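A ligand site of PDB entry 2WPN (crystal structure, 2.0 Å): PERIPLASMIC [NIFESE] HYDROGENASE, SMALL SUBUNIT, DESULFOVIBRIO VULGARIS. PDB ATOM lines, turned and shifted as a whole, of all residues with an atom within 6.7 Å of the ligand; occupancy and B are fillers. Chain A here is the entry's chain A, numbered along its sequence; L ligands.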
ATOM      1  N   ASN A 240     -27.859 -19.354  -5.078  1.00  0.00           N
ATOM      2  CA  ASN A 240     -27.402 -19.603  -3.711  1.00  0.00           C
ATOM      3  C   ASN A 240     -27.264 -18.284  -2.928  1.00  0.00           C
ATOM      4  O   ASN A 240     -26.676 -17.354  -3.441  1.00  0.00           O
ATOM      5  CB  ASN A 240     -26.052 -20.314  -3.792  1.00  0.00           C
ATOM      6  CG  ASN A 240     -25.433 -20.533  -2.435  1.00  0.00           C
ATOM      7  OD1 ASN A 240     -24.541 -19.796  -2.050  1.00  0.00           O
ATOM      8  ND2 ASN A 240     -25.925 -21.531  -1.703  1.00  0.00           N
ATOM      9  N   ILE A 241     -27.812 -18.201  -1.704  1.00  0.00           N
ATOM     10  CA  ILE A 241     -27.745 -16.945  -0.927  1.00  0.00           C
ATOM     11  C   ILE A 241     -26.295 -16.465  -0.701  1.00  0.00           C
ATOM     12  O   ILE A 241     -25.965 -15.288  -0.932  1.00  0.00           O
ATOM     13  CB  ILE A 241     -28.484 -17.069   0.437  1.00  0.00           C
ATOM     14  CG1 ILE A 241     -29.984 -17.264   0.182  1.00  0.00           C
ATOM     15  CG2 ILE A 241     -28.131 -15.862   1.351  1.00  0.00           C
ATOM     16  CD1 ILE A 241     -30.880 -17.286   1.385  1.00  0.00           C
ATOM     17  N   HIS A 242     -25.458 -17.397  -0.246  1.00  0.00           N
ATOM     18  CA  HIS A 242     -24.075 -17.126   0.173  1.00  0.00           C
ATOM     19  C   HIS A 242     -23.207 -16.614  -0.975  1.00  0.00           C
ATOM     20  O   HIS A 242     -22.466 -15.638  -0.797  1.00  0.00           O
ATOM     21  CB  HIS A 242     -23.494 -18.389   0.808  1.00  0.00           C
ATOM     22  CG  HIS A 242     -22.034 -18.308   1.171  1.00  0.00           C
ATOM     23  ND1 HIS A 242     -21.576 -17.651   2.290  1.00  0.00           N
ATOM     24  CD2 HIS A 242     -20.947 -18.849   0.566  1.00  0.00           C
ATOM     25  CE1 HIS A 242     -20.257 -17.789   2.353  1.00  0.00           C
ATOM     26  NE2 HIS A 242     -19.850 -18.508   1.322  1.00  0.00           N
ATOM     27  N   GLU A 243     -23.300 -17.255  -2.144  1.00  0.00           N
ATOM     28  CA  GLU A 243     -22.559 -16.805  -3.356  1.00  0.00           C
ATOM     29  C   GLU A 243     -22.961 -15.393  -3.777  1.00  0.00           C
ATOM     30  O   GLU A 243     -22.214 -14.714  -4.462  1.00  0.00           O
ATOM     31  CB  GLU A 243     -22.808 -17.762  -4.511  1.00  0.00           C
ATOM     32  CG  GLU A 243     -22.086 -19.109  -4.408  1.00  0.00           C
ATOM     33  CD  GLU A 243     -22.630 -20.105  -5.430  1.00  0.00           C
ATOM     34  OE1 GLU A 243     -23.346 -19.676  -6.354  1.00  0.00           O
ATOM     35  OE2 GLU A 243     -22.359 -21.321  -5.304  1.00  0.00           O
ATOM     36  N   CYS A 245     -24.186 -13.089  -1.361  1.00  0.00           N
ATOM     37  CA  CYS A 245     -24.361 -12.374  -0.113  1.00  0.00           C
ATOM     38  C   CYS A 245     -23.444 -11.126  -0.038  1.00  0.00           C
ATOM     39  O   CYS A 245     -22.255 -11.181  -0.433  1.00  0.00           O
ATOM     40  CB  CYS A 245     -24.129 -13.303   1.085  1.00  0.00           C
ATOM     41  SG  CYS A 245     -24.406 -12.494   2.683  1.00  0.00           S
ATOM     42  N   PRO A 246     -23.980  -9.993   0.454  1.00  0.00           N
ATOM     43  CA  PRO A 246     -23.121  -8.813   0.580  1.00  0.00           C
ATOM     44  C   PRO A 246     -21.977  -8.962   1.588  1.00  0.00           C
ATOM     45  O   PRO A 246     -21.048  -8.186   1.518  1.00  0.00           O
ATOM     46  CB  PRO A 246     -24.079  -7.676   1.019  1.00  0.00           C
ATOM     47  CG  PRO A 246     -25.377  -8.272   1.229  1.00  0.00           C
ATOM     48  CD  PRO A 246     -25.394  -9.712   0.788  1.00  0.00           C
ATOM     49  N   TYR A 247     -22.033  -9.954   2.473  1.00  0.00           N
ATOM     50  CA  TYR A 247     -20.967 -10.207   3.445  1.00  0.00           C
ATOM     51  C   TYR A 247     -19.987 -11.282   2.992  1.00  0.00           C
ATOM     52  O   TYR A 247     -19.138 -11.719   3.764  1.00  0.00           O
ATOM     53  CB  TYR A 247     -21.534 -10.505   4.844  1.00  0.00           C
ATOM     54  CG  TYR A 247     -22.632  -9.528   5.213  1.00  0.00           C
ATOM     55  CD1 TYR A 247     -22.326  -8.166   5.439  1.00  0.00           C
ATOM     56  CD2 TYR A 247     -23.980  -9.926   5.276  1.00  0.00           C
ATOM     57  CE1 TYR A 247     -23.347  -7.237   5.728  1.00  0.00           C
ATOM     58  CE2 TYR A 247     -24.984  -9.024   5.567  1.00  0.00           C
ATOM     59  CZ  TYR A 247     -24.674  -7.671   5.792  1.00  0.00           C
ATOM     60  OH  TYR A 247     -25.687  -6.796   6.104  1.00  0.00           O
ATOM     61  N   LEU A 248     -20.074 -11.684   1.727  1.00  0.00           N
ATOM     62  CA  LEU A 248     -19.205 -12.736   1.176  1.00  0.00           C
ATOM     63  C   LEU A 248     -17.710 -12.411   1.401  1.00  0.00           C
ATOM     64  O   LEU A 248     -16.945 -13.269   1.849  1.00  0.00           O
ATOM     65  CB  LEU A 248     -19.540 -13.027  -0.280  1.00  0.00           C
ATOM     66  CG  LEU A 248     -18.737 -14.159  -0.924  1.00  0.00           C
ATOM     67  CD1 LEU A 248     -18.955 -15.474  -0.192  1.00  0.00           C
ATOM     68  CD2 LEU A 248     -19.071 -14.331  -2.399  1.00  0.00           C
ATOM     69  N   ASP A 249     -17.322 -11.166   1.119  1.00  0.00           N
ATOM     70  CA  ASP A 249     -15.958 -10.656   1.389  1.00  0.00           C
ATOM     71  C   ASP A 249     -15.518 -10.902   2.833  1.00  0.00           C
ATOM     72  O   ASP A 249     -14.389 -11.318   3.073  1.00  0.00           O
ATOM     73  CB  ASP A 249     -15.886  -9.159   1.097  1.00  0.00           C
ATOM     74  CG  ASP A 249     -16.741  -8.321   2.098  1.00  0.00           C
ATOM     75  OD1 ASP A 249     -17.938  -8.653   2.316  1.00  0.00           O
ATOM     76  OD2 ASP A 249     -16.207  -7.330   2.656  1.00  0.00           O
ATOM     77  N   LYS A 250     -16.401 -10.649   3.796  1.00  0.00           N
ATOM     78  CA  LYS A 250     -16.059 -10.847   5.208  1.00  0.00           C
ATOM     79  C   LYS A 250     -15.856 -12.331   5.492  1.00  0.00           C
ATOM     80  O   LYS A 250     -14.898 -12.711   6.179  1.00  0.00           O
ATOM     81  CB  LYS A 250     -17.103 -10.261   6.163  1.00  0.00           C
ATOM     82  CG  LYS A 250     -17.395  -8.760   6.001  1.00  0.00           C
ATOM     83  CD  LYS A 250     -16.188  -7.885   6.337  1.00  0.00           C
ATOM     84  CE  LYS A 250     -16.481  -6.437   6.033  1.00  0.00           C
ATOM     85  NZ  LYS A 250     -15.244  -5.637   6.029  1.00  0.00           N
ATOM     86  N   TYR A 251     -16.765 -13.154   4.943  1.00  0.00           N
ATOM     87  CA  TYR A 251     -16.629 -14.604   5.012  1.00  0.00           C
ATOM     88  C   TYR A 251     -15.252 -15.045   4.476  1.00  0.00           C
ATOM     89  O   TYR A 251     -14.534 -15.795   5.155  1.00  0.00           O
ATOM     90  CB  TYR A 251     -17.764 -15.318   4.261  1.00  0.00           C
ATOM     91  CG  TYR A 251     -17.654 -16.841   4.264  1.00  0.00           C
ATOM     92  CD1 TYR A 251     -18.194 -17.603   5.296  1.00  0.00           C
ATOM     93  CD2 TYR A 251     -16.971 -17.497   3.244  1.00  0.00           C
ATOM     94  CE1 TYR A 251     -18.090 -18.992   5.305  1.00  0.00           C
ATOM     95  CE2 TYR A 251     -16.849 -18.907   3.232  1.00  0.00           C
ATOM     96  CZ  TYR A 251     -17.416 -19.635   4.259  1.00  0.00           C
ATOM     97  OH  TYR A 251     -17.300 -21.019   4.265  1.00  0.00           O
ATOM     98  N   ASP A 252     -14.875 -14.584   3.286  1.00  0.00           N
ATOM     99  CA  ASP A 252     -13.568 -14.933   2.701  1.00  0.00           C
ATOM    100  C   ASP A 252     -12.378 -14.392   3.513  1.00  0.00           C
ATOM    101  O   ASP A 252     -11.327 -15.024   3.555  1.00  0.00           O
ATOM    102  CB  ASP A 252     -13.463 -14.553   1.215  1.00  0.00           C
ATOM    103  CG  ASP A 252     -14.400 -15.364   0.332  1.00  0.00           C
ATOM    104  OD1 ASP A 252     -14.639 -16.566   0.636  1.00  0.00           O
ATOM    105  OD2 ASP A 252     -14.923 -14.802  -0.659  1.00  0.00           O
ATOM    106  N   MET A 256     -15.813 -12.619  11.385  1.00  0.00           N
ATOM    107  CA  MET A 256     -17.079 -13.165  11.817  1.00  0.00           C
ATOM    108  C   MET A 256     -17.574 -12.296  12.931  1.00  0.00           C
ATOM    109  O   MET A 256     -16.806 -11.962  13.824  1.00  0.00           O
ATOM    110  CB  MET A 256     -16.843 -14.553  12.364  1.00  0.00           C
ATOM    111  CG  MET A 256     -16.227 -15.453  11.352  1.00  0.00           C
ATOM    112  SD  MET A 256     -17.455 -15.786  10.073  1.00  0.00           S
ATOM    113  CE  MET A 256     -16.491 -16.740   8.878  1.00  0.00           C
ATOM    114  N   GLY A 265     -19.503  -7.884  10.244  1.00  0.00           N
ATOM    115  CA  GLY A 265     -18.922  -9.170   9.874  1.00  0.00           C
ATOM    116  C   GLY A 265     -19.902 -10.193   9.309  1.00  0.00           C
ATOM    117  O   GLY A 265     -21.124 -10.004   9.324  1.00  0.00           O
ATOM    118  N   CYS A 266     -19.345 -11.298   8.814  1.00  0.00           N
ATOM    119  CA  CYS A 266     -20.142 -12.423   8.389  1.00  0.00           C
ATOM    120  C   CYS A 266     -20.874 -13.106   9.550  1.00  0.00           C
ATOM    121  O   CYS A 266     -20.365 -13.180  10.704  1.00  0.00           O
ATOM    122  CB  CYS A 266     -19.230 -13.425   7.674  1.00  0.00           C
ATOM    123  SG  CYS A 266     -20.014 -15.031   7.371  1.00  0.00           S
ATOM    124  N   ARG A 267     -22.070 -13.621   9.237  1.00  0.00           N
ATOM    125  CA  ARG A 267     -22.957 -14.270  10.202  1.00  0.00           C
ATOM    126  C   ARG A 267     -22.711 -15.782  10.343  1.00  0.00           C
ATOM    127  O   ARG A 267     -23.389 -16.483  11.113  1.00  0.00           O
ATOM    128  CB  ARG A 267     -24.418 -13.991   9.841  1.00  0.00           C
ATOM    129  CG  ARG A 267     -24.920 -12.584  10.205  1.00  0.00           C
ATOM    130  CD  ARG A 267     -24.302 -11.478   9.367  1.00  0.00           C
ATOM    131  NE  ARG A 267     -25.229 -10.348   9.232  1.00  0.00           N
ATOM    132  CZ  ARG A 267     -24.834  -9.070   9.090  1.00  0.00           C
ATOM    133  NH1 ARG A 267     -23.558  -8.753   9.064  1.00  0.00           N
ATOM    134  NH2 ARG A 267     -25.742  -8.096   8.974  1.00  0.00           N
ATOM    135  N   TYR A 268     -21.721 -16.282   9.618  1.00  0.00           N
ATOM    136  CA  TYR A 268     -21.493 -17.726   9.624  1.00  0.00           C
ATOM    137  C   TYR A 268     -21.351 -18.302  11.025  1.00  0.00           C
ATOM    138  O   TYR A 268     -22.036 -19.245  11.361  1.00  0.00           O
ATOM    139  CB  TYR A 268     -20.294 -18.096   8.756  1.00  0.00           C
ATOM    140  CG  TYR A 268     -20.018 -19.572   8.720  1.00  0.00           C
ATOM    141  CD1 TYR A 268     -20.666 -20.404   7.801  1.00  0.00           C
ATOM    142  CD2 TYR A 268     -19.111 -20.158   9.611  1.00  0.00           C
ATOM    143  CE1 TYR A 268     -20.390 -21.786   7.773  1.00  0.00           C
ATOM    144  CE2 TYR A 268     -18.848 -21.506   9.610  1.00  0.00           C
ATOM    145  CZ  TYR A 268     -19.485 -22.312   8.684  1.00  0.00           C
ATOM    146  OH  TYR A 268     -19.200 -23.675   8.692  1.00  0.00           O
ATOM    147  N   ASP A 269     -20.479 -17.725  11.858  1.00  0.00           N
ATOM    148  CA  ASP A 269     -20.279 -18.233  13.208  1.00  0.00           C
ATOM    149  C   ASP A 269     -21.549 -18.132  14.098  1.00  0.00           C
ATOM    150  O   ASP A 269     -21.742 -18.927  15.015  1.00  0.00           O
ATOM    151  CB  ASP A 269     -19.092 -17.521  13.868  1.00  0.00           C
ATOM    152  CG  ASP A 269     -17.745 -18.148  13.519  1.00  0.00           C
ATOM    153  OD1 ASP A 269     -17.669 -19.114  12.735  1.00  0.00           O
ATOM    154  OD2 ASP A 269     -16.742 -17.667  14.068  1.00  0.00           O
ATOM    155  N   CYS A 272     -25.421 -18.809  10.418  1.00  0.00           N
ATOM    156  CA  CYS A 272     -25.953 -18.553   9.067  1.00  0.00           C
ATOM    157  C   CYS A 272     -25.916 -19.767   8.161  1.00  0.00           C
ATOM    158  O   CYS A 272     -24.842 -20.362   7.947  1.00  0.00           O
ATOM    159  CB  CYS A 272     -25.178 -17.430   8.371  1.00  0.00           C
ATOM    160  SG  CYS A 272     -26.056 -16.872   6.897  1.00  0.00           S
ATOM    161  N   LYS A 273     -27.071 -20.080   7.588  1.00  0.00           N
ATOM    162  CA  LYS A 273     -27.205 -21.236   6.717  1.00  0.00           C
ATOM    163  C   LYS A 273     -27.194 -20.852   5.223  1.00  0.00           C
ATOM    164  O   LYS A 273     -27.415 -21.707   4.354  1.00  0.00           O
ATOM    165  CB  LYS A 273     -28.436 -22.070   7.095  1.00  0.00           C
ATOM    166  CG  LYS A 273     -28.365 -22.760   8.472  1.00  0.00           C
ATOM    167  CD  LYS A 273     -26.972 -23.355   8.828  1.00  0.00           C
ATOM    168  CE  LYS A 273     -26.929 -23.905  10.274  1.00  0.00           C
ATOM    169  NZ  LYS A 273     -27.498 -23.021  11.347  1.00  0.00           N
ATOM    170  N   GLY A 274     -26.909 -19.575   4.937  1.00  0.00           N
ATOM    171  CA  GLY A 274     -26.697 -19.077   3.584  1.00  0.00           C
ATOM    172  C   GLY A 274     -25.886 -19.992   2.651  1.00  0.00           C
ATOM    173  O   GLY A 274     -26.290 -20.182   1.495  1.00  0.00           O
ATOM    174  N   PRO A 275     -24.737 -20.556   3.135  1.00  0.00           N
ATOM    175  CA  PRO A 275     -23.965 -21.452   2.270  1.00  0.00           C
ATOM    176  C   PRO A 275     -24.740 -22.627   1.669  1.00  0.00           C
ATOM    177  O   PRO A 275     -24.383 -23.077   0.578  1.00  0.00           O
ATOM    178  CB  PRO A 275     -22.840 -21.966   3.200  1.00  0.00           C
ATOM    179  CG  PRO A 275     -22.563 -20.804   4.113  1.00  0.00           C
ATOM    180  CD  PRO A 275     -24.009 -20.294   4.408  1.00  0.00           C
ATOM    181  N   TRP A 292     -34.078  -8.277   5.616  1.00  0.00           N
ATOM    182  CA  TRP A 292     -34.058  -9.706   5.313  1.00  0.00           C
ATOM    183  C   TRP A 292     -33.256 -10.489   6.377  1.00  0.00           C
ATOM    184  O   TRP A 292     -32.525  -9.890   7.192  1.00  0.00           O
ATOM    185  CB  TRP A 292     -33.574  -9.945   3.871  1.00  0.00           C
ATOM    186  CG  TRP A 292     -32.143  -9.693   3.624  1.00  0.00           C
ATOM    187  CD1 TRP A 292     -31.474  -8.510   3.755  1.00  0.00           C
ATOM    188  CD2 TRP A 292     -31.178 -10.657   3.176  1.00  0.00           C
ATOM    189  NE1 TRP A 292     -30.146  -8.683   3.442  1.00  0.00           N
ATOM    190  CE2 TRP A 292     -29.939  -9.989   3.065  1.00  0.00           C
ATOM    191  CE3 TRP A 292     -31.240 -12.035   2.852  1.00  0.00           C
ATOM    192  CZ2 TRP A 292     -28.774 -10.644   2.666  1.00  0.00           C
ATOM    193  CZ3 TRP A 292     -30.065 -12.684   2.436  1.00  0.00           C
ATOM    194  CH2 TRP A 292     -28.861 -11.988   2.350  1.00  0.00           C
ATOM    195  N   VAL A 294     -30.632 -12.306   6.705  1.00  0.00           N
ATOM    196  CA  VAL A 294     -29.184 -12.192   6.900  1.00  0.00           C
ATOM    197  C   VAL A 294     -28.754 -10.818   7.441  1.00  0.00           C
ATOM    198  O   VAL A 294     -27.882 -10.735   8.311  1.00  0.00           O
ATOM    199  CB  VAL A 294     -28.371 -12.623   5.646  1.00  0.00           C
ATOM    200  CG1 VAL A 294     -26.899 -12.354   5.848  1.00  0.00           C
ATOM    201  CG2 VAL A 294     -28.610 -14.086   5.316  1.00  0.00           C
ATOM    202  N   ALA A 297     -30.426 -10.952  11.282  1.00  0.00           N
ATOM    203  CA  ALA A 297     -29.972 -12.000  12.195  1.00  0.00           C
ATOM    204  C   ALA A 297     -29.149 -13.076  11.435  1.00  0.00           C
ATOM    205  O   ALA A 297     -27.996 -12.853  11.152  1.00  0.00           O
ATOM    206  CB  ALA A 297     -31.195 -12.630  12.982  1.00  0.00           C
ATOM    207  N   CYS A 299     -29.638 -16.508   8.279  1.00  0.00           N
ATOM    208  CA  CYS A 299     -30.493 -17.363   7.432  1.00  0.00           C
ATOM    209  C   CYS A 299     -30.625 -18.708   8.121  1.00  0.00           C
ATOM    210  O   CYS A 299     -29.637 -19.231   8.630  1.00  0.00           O
ATOM    211  CB  CYS A 299     -29.883 -17.569   6.031  1.00  0.00           C
ATOM    212  SG  CYS A 299     -30.820 -18.690   4.955  1.00  0.00           S
HETATM  213 FE1  LIG L   1     -24.263 -16.060   5.682  1.00  0.00          FE
HETATM  214 FE2  LIG L   1     -21.722 -15.046   5.818  1.00  0.00          FE
HETATM  215 FE3  LIG L   1     -23.470 -14.149   3.969  1.00  0.00          FE
HETATM  216 FE4  LIG L   1     -22.463 -16.567   3.690  1.00  0.00          FE
HETATM  217  S1  LIG L   1     -21.270 -14.593   3.602  1.00  0.00           S
HETATM  218  S2  LIG L   1     -24.684 -16.031   3.423  1.00  0.00           S
HETATM  219  S3  LIG L   1     -22.321 -17.277   5.893  1.00  0.00           S
HETATM  220  S4  LIG L   1     -23.659 -13.886   6.256  1.00  0.00           S
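A ring nitrogen (ND1) of His 242 binds an iron atom (FE4) of the ligand (2.0 Å). An iron atom (FE3) of the ligand is bound by the side-chain sulfur (SG) of Cys 245, at 2.3 Å. An iron atom (FE2) of the ligand is bound by the side-chain sulfur of Cys 266. The side-chain sulfur (SG) of Cys 272 is bound to an iron atom (FE1) of the ligand (2.3 Å). S4 of the ligand sits close to N of Arg 267 (3.4 Å). N of Leu 248 sits close to S1 of the ligand (3.7 Å).
SG of Cys 245 sits close to N of Tyr 247, 3.5 Å away. The side-chain sulfur (SG) of Cys 266 sits close to the backbone NH (N) of Tyr 268, at 3.1 Å. The side-chain sulfur (SD) of Met 256 sits close to the side-chain sulfur (SG) of Cys 266 (3.8 Å). The backbone NH (N) of Cys 272 sits at hydrogen-bond distance from the backbone carbonyl oxygen (O) of Arg 267 (3.2 Å). The guanidinium group (NH2) of Arg 267 sits at hydrogen-bond distance from the side-chain hydroxyl (OH) of Tyr 247, at 3.2 Å. The guanidinium group (NE) of Arg 267 is in hydrogen-bond range of the backbone carbonyl oxygen (O) of Val 294, 2.8 Å away. The guanidinium group (NH1) of Arg 267 sits at hydrogen-bond distance from the backbone carbonyl oxygen (O) of Gly 265 (2.7 Å). The side-chain amide nitrogen (ND2) of Asn 240 is in hydrogen-bond range of the backbone carbonyl oxygen (O) of Gly 274.
O of Tyr 247 lies close to S1 of the ligand. Tyr 251 touches the ligand. Tyr 268 touches the ligand. Gly 274 touches the ligand. Pro 275 touches the ligand. Val 294 touches the ligand. Hydrophobic or aromatic side chains that line the ligand: His 242, Tyr 251, Tyr 268, Pro 275 and Val 294. Of the 26 residues printed, 12 come within 4 Å of the ligand. Along chain A the residues within 4 Å of the ligand span positions 242 to 294.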
